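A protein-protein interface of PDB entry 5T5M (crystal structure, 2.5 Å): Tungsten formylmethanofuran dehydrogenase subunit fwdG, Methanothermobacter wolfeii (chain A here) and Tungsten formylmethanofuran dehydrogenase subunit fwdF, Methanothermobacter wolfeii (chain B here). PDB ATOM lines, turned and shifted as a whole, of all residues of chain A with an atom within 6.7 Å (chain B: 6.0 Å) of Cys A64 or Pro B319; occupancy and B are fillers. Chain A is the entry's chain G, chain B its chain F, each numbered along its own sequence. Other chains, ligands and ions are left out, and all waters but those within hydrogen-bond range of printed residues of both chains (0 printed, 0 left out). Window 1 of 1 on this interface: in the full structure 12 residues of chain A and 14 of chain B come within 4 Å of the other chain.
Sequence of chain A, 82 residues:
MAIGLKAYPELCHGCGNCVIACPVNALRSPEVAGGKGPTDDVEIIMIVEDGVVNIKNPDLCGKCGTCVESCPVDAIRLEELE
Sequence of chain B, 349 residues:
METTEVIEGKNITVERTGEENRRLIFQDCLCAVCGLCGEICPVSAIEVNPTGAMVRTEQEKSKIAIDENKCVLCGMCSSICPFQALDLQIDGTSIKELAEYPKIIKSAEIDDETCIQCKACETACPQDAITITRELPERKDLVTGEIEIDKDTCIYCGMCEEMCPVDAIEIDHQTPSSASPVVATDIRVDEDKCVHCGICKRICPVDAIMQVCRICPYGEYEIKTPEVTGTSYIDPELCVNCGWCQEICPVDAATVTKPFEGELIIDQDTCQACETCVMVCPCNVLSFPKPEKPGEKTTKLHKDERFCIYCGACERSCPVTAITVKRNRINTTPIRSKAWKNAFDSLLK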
ATOM      1  N   CYS A  22      31.869  12.385  -1.303  1.00  0.00           N
ATOM      2  CA  CYS A  22      30.619  13.050  -0.984  1.00  0.00           C
ATOM      3  C   CYS A  22      30.123  13.874  -2.170  1.00  0.00           C
ATOM      4  O   CYS A  22      30.830  14.790  -2.610  1.00  0.00           O
ATOM      5  CB  CYS A  22      30.803  13.946   0.232  1.00  0.00           C
ATOM      6  SG  CYS A  22      29.430  15.099   0.456  1.00  0.00           S
ATOM      7  N   PRO A  23      28.928  13.604  -2.704  1.00  0.00           N
ATOM      8  CA  PRO A  23      28.441  14.407  -3.839  1.00  0.00           C
ATOM      9  C   PRO A  23      28.149  15.852  -3.468  1.00  0.00           C
ATOM     10  O   PRO A  23      28.286  16.745  -4.315  1.00  0.00           O
ATOM     11  CB  PRO A  23      27.170  13.660  -4.279  1.00  0.00           C
ATOM     12  CG  PRO A  23      26.746  12.883  -3.088  1.00  0.00           C
ATOM     13  CD  PRO A  23      28.010  12.501  -2.375  1.00  0.00           C
ATOM     14  N   VAL A  24      27.758  16.109  -2.218  1.00  0.00           N
ATOM     15  CA  VAL A  24      27.535  17.480  -1.772  1.00  0.00           C
ATOM     16  C   VAL A  24      28.847  18.252  -1.761  1.00  0.00           C
ATOM     17  O   VAL A  24      28.926  19.382  -2.262  1.00  0.00           O
ATOM     18  CB  VAL A  24      26.871  17.485  -0.386  1.00  0.00           C
ATOM     19  CG1 VAL A  24      26.567  18.900   0.057  1.00  0.00           C
ATOM     20  CG2 VAL A  24      25.603  16.649  -0.399  1.00  0.00           C
ATOM     21  N   LEU A  27      29.928  18.838  -5.413  1.00  0.00           N
ATOM     22  CA  LEU A  27      29.168  19.869  -6.110  1.00  0.00           C
ATOM     23  C   LEU A  27      29.665  21.256  -5.737  1.00  0.00           C
ATOM     24  O   LEU A  27      29.728  22.154  -6.588  1.00  0.00           O
ATOM     25  CB  LEU A  27      27.682  19.725  -5.790  1.00  0.00           C
ATOM     26  CG  LEU A  27      26.743  20.730  -6.465  1.00  0.00           C
ATOM     27  CD1 LEU A  27      26.876  20.679  -7.974  1.00  0.00           C
ATOM     28  CD2 LEU A  27      25.311  20.466  -6.067  1.00  0.00           C
ATOM     29  N   ILE A  45      30.286  19.638   3.976  1.00  0.00           N
ATOM     30  CA  ILE A  45      29.786  18.876   5.114  1.00  0.00           C
ATOM     31  C   ILE A  45      30.908  18.596   6.100  1.00  0.00           C
ATOM     32  O   ILE A  45      30.747  18.764   7.314  1.00  0.00           O
ATOM     33  CB  ILE A  45      29.124  17.569   4.648  1.00  0.00           C
ATOM     34  CG1 ILE A  45      28.091  17.864   3.554  1.00  0.00           C
ATOM     35  CG2 ILE A  45      28.525  16.842   5.849  1.00  0.00           C
ATOM     36  CD1 ILE A  45      26.968  16.860   3.443  1.00  0.00           C
ATOM     37  N   LEU A  60      23.666  20.009   5.670  1.00  0.00           N
ATOM     38  CA  LEU A  60      23.692  19.761   4.229  1.00  0.00           C
ATOM     39  C   LEU A  60      23.664  18.281   3.879  1.00  0.00           C
ATOM     40  O   LEU A  60      23.409  17.931   2.718  1.00  0.00           O
ATOM     41  CB  LEU A  60      24.946  20.395   3.615  1.00  0.00           C
ATOM     42  CG  LEU A  60      25.109  21.890   3.911  1.00  0.00           C
ATOM     43  CD1 LEU A  60      26.429  22.422   3.355  1.00  0.00           C
ATOM     44  CD2 LEU A  60      23.933  22.668   3.346  1.00  0.00           C
ATOM     45  N   CYS A  61      23.932  17.413   4.849  1.00  0.00           N
ATOM     46  CA  CYS A  61      23.940  15.981   4.601  1.00  0.00           C
ATOM     47  C   CYS A  61      22.551  15.472   4.232  1.00  0.00           C
ATOM     48  O   CYS A  61      21.561  15.778   4.904  1.00  0.00           O
ATOM     49  CB  CYS A  61      24.459  15.271   5.843  1.00  0.00           C
ATOM     50  SG  CYS A  61      24.162  13.520   5.862  1.00  0.00           S
ATOM     51  N   GLY A  62      22.485  14.696   3.153  1.00  0.00           N
ATOM     52  CA  GLY A  62      21.287  14.003   2.730  1.00  0.00           C
ATOM     53  C   GLY A  62      21.234  12.546   3.134  1.00  0.00           C
ATOM     54  O   GLY A  62      20.347  11.821   2.669  1.00  0.00           O
ATOM     55  N   LYS A  63      22.152  12.094   3.982  1.00  0.00           N
ATOM     56  CA  LYS A  63      22.175  10.726   4.491  1.00  0.00           C
ATOM     57  C   LYS A  63      22.034   9.706   3.358  1.00  0.00           C
ATOM     58  O   LYS A  63      21.139   8.859   3.355  1.00  0.00           O
ATOM     59  CB  LYS A  63      21.081  10.521   5.538  1.00  0.00           C
ATOM     60  CG  LYS A  63      21.159  11.472   6.719  1.00  0.00           C
ATOM     61  CD  LYS A  63      20.331  12.729   6.489  1.00  0.00           C
ATOM     62  CE  LYS A  63      20.636  13.790   7.530  1.00  0.00           C
ATOM     63  NZ  LYS A  63      19.752  14.972   7.369  1.00  0.00           N
ATOM     64  N   CYS A  64      22.938   9.785   2.385  1.00  0.00           N
ATOM     65  CA  CYS A  64      22.882   8.819   1.301  1.00  0.00           C
ATOM     66  C   CYS A  64      23.777   7.616   1.554  1.00  0.00           C
ATOM     67  O   CYS A  64      23.502   6.534   1.030  1.00  0.00           O
ATOM     68  CB  CYS A  64      23.248   9.478  -0.031  1.00  0.00           C
ATOM     69  SG  CYS A  64      24.973   9.923  -0.260  1.00  0.00           S
ATOM     70  N   GLY A  65      24.817   7.779   2.370  1.00  0.00           N
ATOM     71  CA  GLY A  65      25.672   6.678   2.763  1.00  0.00           C
ATOM     72  C   GLY A  65      26.886   6.458   1.890  1.00  0.00           C
ATOM     73  O   GLY A  65      27.604   5.471   2.099  1.00  0.00           O
ATOM     74  N   THR A  66      27.150   7.343   0.926  1.00  0.00           N
ATOM     75  CA  THR A  66      28.304   7.152   0.055  1.00  0.00           C
ATOM     76  C   THR A  66      29.602   7.213   0.854  1.00  0.00           C
ATOM     77  O   THR A  66      30.464   6.341   0.727  1.00  0.00           O
ATOM     78  CB  THR A  66      28.305   8.206  -1.050  1.00  0.00           C
ATOM     79  OG1 THR A  66      27.095   8.105  -1.816  1.00  0.00           O
ATOM     80  CG2 THR A  66      29.496   8.021  -1.963  1.00  0.00           C
ATOM     81  N   CYS A  67      29.750   8.245   1.688  1.00  0.00           N
ATOM     82  CA  CYS A  67      30.938   8.378   2.521  1.00  0.00           C
ATOM     83  C   CYS A  67      31.138   7.147   3.389  1.00  0.00           C
ATOM     84  O   CYS A  67      32.270   6.680   3.561  1.00  0.00           O
ATOM     85  CB  CYS A  67      30.823   9.628   3.392  1.00  0.00           C
ATOM     86  SG  CYS A  67      29.665   9.485   4.785  1.00  0.00           S
ATOM     87  N   GLU A  69      30.294   4.037   2.838  1.00  0.00           N
ATOM     88  CA  GLU A  69      30.745   2.890   2.060  1.00  0.00           C
ATOM     89  C   GLU A  69      32.155   3.069   1.516  1.00  0.00           C
ATOM     90  O   GLU A  69      32.744   2.100   1.029  1.00  0.00           O
ATOM     91  CB  GLU A  69      29.770   2.638   0.908  1.00  0.00           C
ATOM     92  CG  GLU A  69      29.543   1.159   0.568  1.00  0.00           C
ATOM     93  CD  GLU A  69      28.057   0.810   0.412  1.00  0.00           C
ATOM     94  OE1 GLU A  69      27.262   1.729   0.116  1.00  0.00           O
ATOM     95  OE2 GLU A  69      27.687  -0.375   0.593  1.00  0.00           O
ATOM     96  N   LEU A  78      26.333   6.603   9.549  1.00  0.00           N
ATOM     97  CA  LEU A  78      25.007   7.199   9.612  1.00  0.00           C
ATOM     98  C   LEU A  78      24.199   6.428  10.645  1.00  0.00           C
ATOM     99  O   LEU A  78      23.994   5.218  10.493  1.00  0.00           O
ATOM    100  CB  LEU A  78      24.321   7.152   8.248  1.00  0.00           C
ATOM    101  CG  LEU A  78      24.818   8.127   7.182  1.00  0.00           C
ATOM    102  CD1 LEU A  78      24.216   7.790   5.828  1.00  0.00           C
ATOM    103  CD2 LEU A  78      24.471   9.556   7.559  1.00  0.00           C
ATOM    104  N   PRO B  50      15.924   8.251   5.668  1.00  0.00           N
ATOM    105  CA  PRO B  50      16.571   8.593   4.393  1.00  0.00           C
ATOM    106  C   PRO B  50      16.736   7.376   3.497  1.00  0.00           C
ATOM    107  O   PRO B  50      17.188   6.319   3.935  1.00  0.00           O
ATOM    108  CB  PRO B  50      17.927   9.161   4.830  1.00  0.00           C
ATOM    109  CG  PRO B  50      17.697   9.668   6.204  1.00  0.00           C
ATOM    110  CD  PRO B  50      16.700   8.737   6.821  1.00  0.00           C
ATOM    111  N   THR B  51      16.384   7.548   2.223  1.00  0.00           N
ATOM    112  CA  THR B  51      16.349   6.419   1.298  1.00  0.00           C
ATOM    113  C   THR B  51      17.743   5.848   1.055  1.00  0.00           C
ATOM    114  O   THR B  51      17.912   4.626   0.984  1.00  0.00           O
ATOM    115  CB  THR B  51      15.712   6.854  -0.016  1.00  0.00           C
ATOM    116  OG1 THR B  51      14.448   7.483   0.251  1.00  0.00           O
ATOM    117  CG2 THR B  51      15.515   5.646  -0.956  1.00  0.00           C
ATOM    118  N   GLY B  52      18.753   6.710   0.924  1.00  0.00           N
ATOM    119  CA  GLY B  52      20.107   6.216   0.730  1.00  0.00           C
ATOM    120  C   GLY B  52      20.616   5.421   1.918  1.00  0.00           C
ATOM    121  O   GLY B  52      21.109   4.302   1.763  1.00  0.00           O
ATOM    122  N   ALA B  53      20.484   5.982   3.125  1.00  0.00           N
ATOM    123  CA  ALA B  53      21.055   5.354   4.317  1.00  0.00           C
ATOM    124  C   ALA B  53      20.423   3.999   4.601  1.00  0.00           C
ATOM    125  O   ALA B  53      21.097   3.082   5.081  1.00  0.00           O
ATOM    126  CB  ALA B  53      20.888   6.273   5.529  1.00  0.00           C
ATOM    127  N   ARG B  56      22.182   1.614   1.674  1.00  0.00           N
ATOM    128  CA  ARG B  56      23.626   1.468   1.523  1.00  0.00           C
ATOM    129  C   ARG B  56      24.366   1.205   2.832  1.00  0.00           C
ATOM    130  O   ARG B  56      25.539   0.824   2.787  1.00  0.00           O
ATOM    131  CB  ARG B  56      24.211   2.729   0.873  1.00  0.00           C
ATOM    132  CG  ARG B  56      23.666   3.007  -0.515  1.00  0.00           C
ATOM    133  CD  ARG B  56      24.416   4.137  -1.202  1.00  0.00           C
ATOM    134  NE  ARG B  56      25.815   3.800  -1.417  1.00  0.00           N
ATOM    135  CZ  ARG B  56      26.631   4.453  -2.236  1.00  0.00           C
ATOM    136  NH1 ARG B  56      27.889   4.050  -2.361  1.00  0.00           N
ATOM    137  NH2 ARG B  56      26.196   5.498  -2.936  1.00  0.00           N
ATOM    138  N   THR B  57      23.732   1.427   3.980  1.00  0.00           N
ATOM    139  CA  THR B  57      24.324   1.173   5.286  1.00  0.00           C
ATOM    140  C   THR B  57      23.429   0.224   6.072  1.00  0.00           C
ATOM    141  O   THR B  57      22.253   0.030   5.752  1.00  0.00           O
ATOM    142  CB  THR B  57      24.516   2.470   6.090  1.00  0.00           C
ATOM    143  OG1 THR B  57      23.247   2.945   6.551  1.00  0.00           O
ATOM    144  CG2 THR B  57      25.166   3.556   5.254  1.00  0.00           C
ATOM    145  N   CYS B 274      27.575   9.647  -7.366  1.00  0.00           N
ATOM    146  CA  CYS B 274      27.828   8.896  -6.145  1.00  0.00           C
ATOM    147  C   CYS B 274      27.141   7.541  -6.159  1.00  0.00           C
ATOM    148  O   CYS B 274      27.356   6.747  -5.241  1.00  0.00           O
ATOM    149  CB  CYS B 274      27.374   9.695  -4.920  1.00  0.00           C
ATOM    150  SG  CYS B 274      25.605   9.624  -4.623  1.00  0.00           S
ATOM    151  N   THR B 276      24.227   6.522  -5.560  1.00  0.00           N
ATOM    152  CA  THR B 276      23.176   6.218  -4.591  1.00  0.00           C
ATOM    153  C   THR B 276      21.867   5.871  -5.289  1.00  0.00           C
ATOM    154  O   THR B 276      21.254   4.833  -5.012  1.00  0.00           O
ATOM    155  CB  THR B 276      22.971   7.407  -3.649  1.00  0.00           C
ATOM    156  OG1 THR B 276      24.143   7.606  -2.853  1.00  0.00           O
ATOM    157  CG2 THR B 276      21.780   7.172  -2.731  1.00  0.00           C
ATOM    158  N   GLU B 315      14.825  10.224  -6.568  1.00  0.00           N
ATOM    159  CA  GLU B 315      14.784  11.656  -6.272  1.00  0.00           C
ATOM    160  C   GLU B 315      14.955  11.907  -4.784  1.00  0.00           C
ATOM    161  O   GLU B 315      15.708  12.797  -4.371  1.00  0.00           O
ATOM    162  CB  GLU B 315      13.464  12.260  -6.758  1.00  0.00           C
ATOM    163  CG  GLU B 315      13.027  13.514  -6.013  1.00  0.00           C
ATOM    164  CD  GLU B 315      11.887  14.247  -6.711  1.00  0.00           C
ATOM    165  OE1 GLU B 315      12.055  15.448  -7.015  1.00  0.00           O
ATOM    166  OE2 GLU B 315      10.829  13.627  -6.963  1.00  0.00           O
ATOM    167  N   ARG B 316      14.257  11.123  -3.966  1.00  0.00           N
ATOM    168  CA  ARG B 316      14.366  11.233  -2.517  1.00  0.00           C
ATOM    169  C   ARG B 316      15.773  10.940  -2.009  1.00  0.00           C
ATOM    170  O   ARG B 316      16.196  11.517  -1.002  1.00  0.00           O
ATOM    171  CB  ARG B 316      13.374  10.273  -1.882  1.00  0.00           C
ATOM    172  CG  ARG B 316      13.240  10.413  -0.410  1.00  0.00           C
ATOM    173  CD  ARG B 316      11.964   9.735   0.051  1.00  0.00           C
ATOM    174  NE  ARG B 316      11.602  10.163   1.392  1.00  0.00           N
ATOM    175  CZ  ARG B 316      12.164   9.691   2.492  1.00  0.00           C
ATOM    176  NH1 ARG B 316      11.769  10.150   3.669  1.00  0.00           N
ATOM    177  NH2 ARG B 316      13.117   8.759   2.414  1.00  0.00           N
ATOM    178  N   SER B 317      16.505  10.036  -2.662  1.00  0.00           N
ATOM    179  CA  SER B 317      17.798   9.625  -2.139  1.00  0.00           C
ATOM    180  C   SER B 317      18.913  10.588  -2.515  1.00  0.00           C
ATOM    181  O   SER B 317      19.986  10.542  -1.904  1.00  0.00           O
ATOM    182  CB  SER B 317      18.142   8.219  -2.635  1.00  0.00           C
ATOM    183  OG  SER B 317      18.588   8.236  -3.982  1.00  0.00           O
ATOM    184  N   CYS B 318      18.693  11.458  -3.492  1.00  0.00           N
ATOM    185  CA  CYS B 318      19.792  12.236  -4.050  1.00  0.00           C
ATOM    186  C   CYS B 318      20.099  13.450  -3.180  1.00  0.00           C
ATOM    187  O   CYS B 318      19.262  14.353  -3.076  1.00  0.00           O
ATOM    188  CB  CYS B 318      19.468  12.680  -5.462  1.00  0.00           C
ATOM    189  SG  CYS B 318      20.643  13.899  -6.077  1.00  0.00           S
ATOM    190  N   PRO B 319      21.284  13.529  -2.569  1.00  0.00           N
ATOM    191  CA  PRO B 319      21.566  14.653  -1.669  1.00  0.00           C
ATOM    192  C   PRO B 319      21.763  15.981  -2.377  1.00  0.00           C
ATOM    193  O   PRO B 319      21.711  17.022  -1.710  1.00  0.00           O
ATOM    194  CB  PRO B 319      22.845  14.211  -0.940  1.00  0.00           C
ATOM    195  CG  PRO B 319      23.455  13.224  -1.816  1.00  0.00           C
ATOM    196  CD  PRO B 319      22.372  12.541  -2.575  1.00  0.00           C
ATOM    197  N   VAL B 320      21.978  15.993  -3.688  1.00  0.00           N
ATOM    198  CA  VAL B 320      22.141  17.231  -4.437  1.00  0.00           C
ATOM    199  C   VAL B 320      20.938  17.502  -5.338  1.00  0.00           C
ATOM    200  O   VAL B 320      20.988  18.397  -6.187  1.00  0.00           O
ATOM    201  CB  VAL B 320      23.453  17.228  -5.246  1.00  0.00           C
ATOM    202  CG1 VAL B 320      24.663  17.206  -4.310  1.00  0.00           C
ATOM    203  CG2 VAL B 320      23.499  16.049  -6.202  1.00  0.00           C
ATOM    204  N   THR B 321      19.852  16.754  -5.170  1.00  0.00           N
ATOM    205  CA  THR B 321      18.621  16.984  -5.922  1.00  0.00           C
ATOM    206  C   THR B 321      18.880  17.063  -7.430  1.00  0.00           C
ATOM    207  O   THR B 321      18.386  17.953  -8.125  1.00  0.00           O
ATOM    208  CB  THR B 321      17.934  18.251  -5.421  1.00  0.00           C
ATOM    209  OG1 THR B 321      18.069  18.321  -3.995  1.00  0.00           O
ATOM    210  CG2 THR B 321      16.470  18.237  -5.774  1.00  0.00           C
ATOM    211  N   ALA B 322      19.655  16.106  -7.954  1.00  0.00           N
ATOM    212  CA  ALA B 322      19.915  16.094  -9.386  1.00  0.00           C
ATOM    213  C   ALA B 322      18.811  15.409 -10.182  1.00  0.00           C
ATOM    214  O   ALA B 322      18.735  15.604 -11.403  1.00  0.00           O
ATOM    215  CB  ALA B 322      21.245  15.413  -9.679  1.00  0.00           C
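Cys A22 touches none of the printed residues of chain B. Of chain B, only Gly B52 (3.2 Å), Ala B53 (3.7 Å), Arg B56 (3.4 Å), Thr B276 (3.5 Å), Ser B317 (3.9 Å) and Pro B319 (3.95 Å) come within 4 Å of Cys A64. Printed residues of chain B within 4 Å of Thr A66: Arg B56, Cys B274 and Thr B276. Of the printed residues of chain B, Glu A69 touches Arg B56 (3.0 Å). Of the printed residues of chain A, Gly B52 touches Lys A63 and Cys A64. Printed residues of chain A within 4 Å of Pro B319: Pro A23 (3.5 Å), Val A24 (3.7 Å), Gly A62 (3.99 Å) and Cys A64 (3.95 Å). Thr B321 touches none of the printed residues of chain A. The nearest residue of chain B that does not touch Cys A64 is Cys B274 (4.4 Å). The nearest printed residue of chain A that does not touch Pro B319 is Leu A60 (4.8 Å). The nearest printed residue of chain A that does not touch Thr B276 is Gly A65 (5.3 Å).
Hydrophobic or aromatic side chains of chain A that line the printed part of chain B: Pro A23, Val A24, Leu A27 and Leu A78. Printed residues of chain B that touch a printed residue of chain A: Pro B50, Gly B52, Ala B53, Arg B56, Cys B274, Thr B276, Ser B317, Pro B319 and Val B320. Along chain B the printed residues that touch a printed residue of chain A span positions 50 to 320.
The backbone NH (N) of Ala B53 is in hydrogen-bond range of the backbone carbonyl oxygen (O) of Lys A63 (3.0 Å). The guanidinium group of Arg B56 lies within hydrogen-bond range of the side-chain hydroxyl of Thr A66, 3.0 Å away. OE1 of Glu A69 lies within salt-bridge range of NE of Arg B56, at 3.0 Å. SG of Cys B274 sits close to OG1 of Thr A66 (3.5 Å). The side-chain hydroxyl of Thr B276 lies close to the side-chain sulfur of Cys A64 (3.6 Å). The side-chain hydroxyl (OG1) of Thr A66 lies within hydrogen-bond range of the side-chain hydroxyl (OG1) of Thr B276 (3.2 Å). The backbone carbonyl oxygen (O) of Cys A64 lies close to the backbone carbonyl oxygen (O) of Gly B52 (3.4 Å).
The backbone carbonyl oxygen (O) of Ala B53 lies within hydrogen-bond range of the side-chain hydroxyl (OG1) of Thr B57 (2.6 Å). SG of Cys B274 sits close to OG1 of Thr B276 (3.1 Å). The side-chain sulfur (SG) of Cys B318 lies close to the backbone NH (N) of Val B320, 3.4 Å away. The side-chain sulfur (SG) of Cys A22 lies close to the backbone NH (N) of Val A24, at 3.3 Å. The side-chain amino group (NZ) of Lys A63 is in hydrogen-bond range of the backbone carbonyl oxygen (O) of Cys A61, 3.2 Å away. SG of Cys A64 lies close to OG1 of Thr A66 (3.2 Å).
CB of Cys B274 touches CG of Pro A23, at 3.7 Å. Pro B319 touches Pro A23. Pro B319 touches Val A24 (CB to CG2, 3.7 Å). Val A24 touches Val B320 (CA to CG1, 3.8 Å). Leu A27 touches Val B320 (CD2 to CG1, 3.8 Å). Pro B319 touches Gly A62. Lys A63 touches Pro B50. Ala B53 touches Cys A64 (N to O, 3.7 Å). CD of Arg B56 touches O of Cys A64, at 3.4 Å. Ser B317 touches Cys A64.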
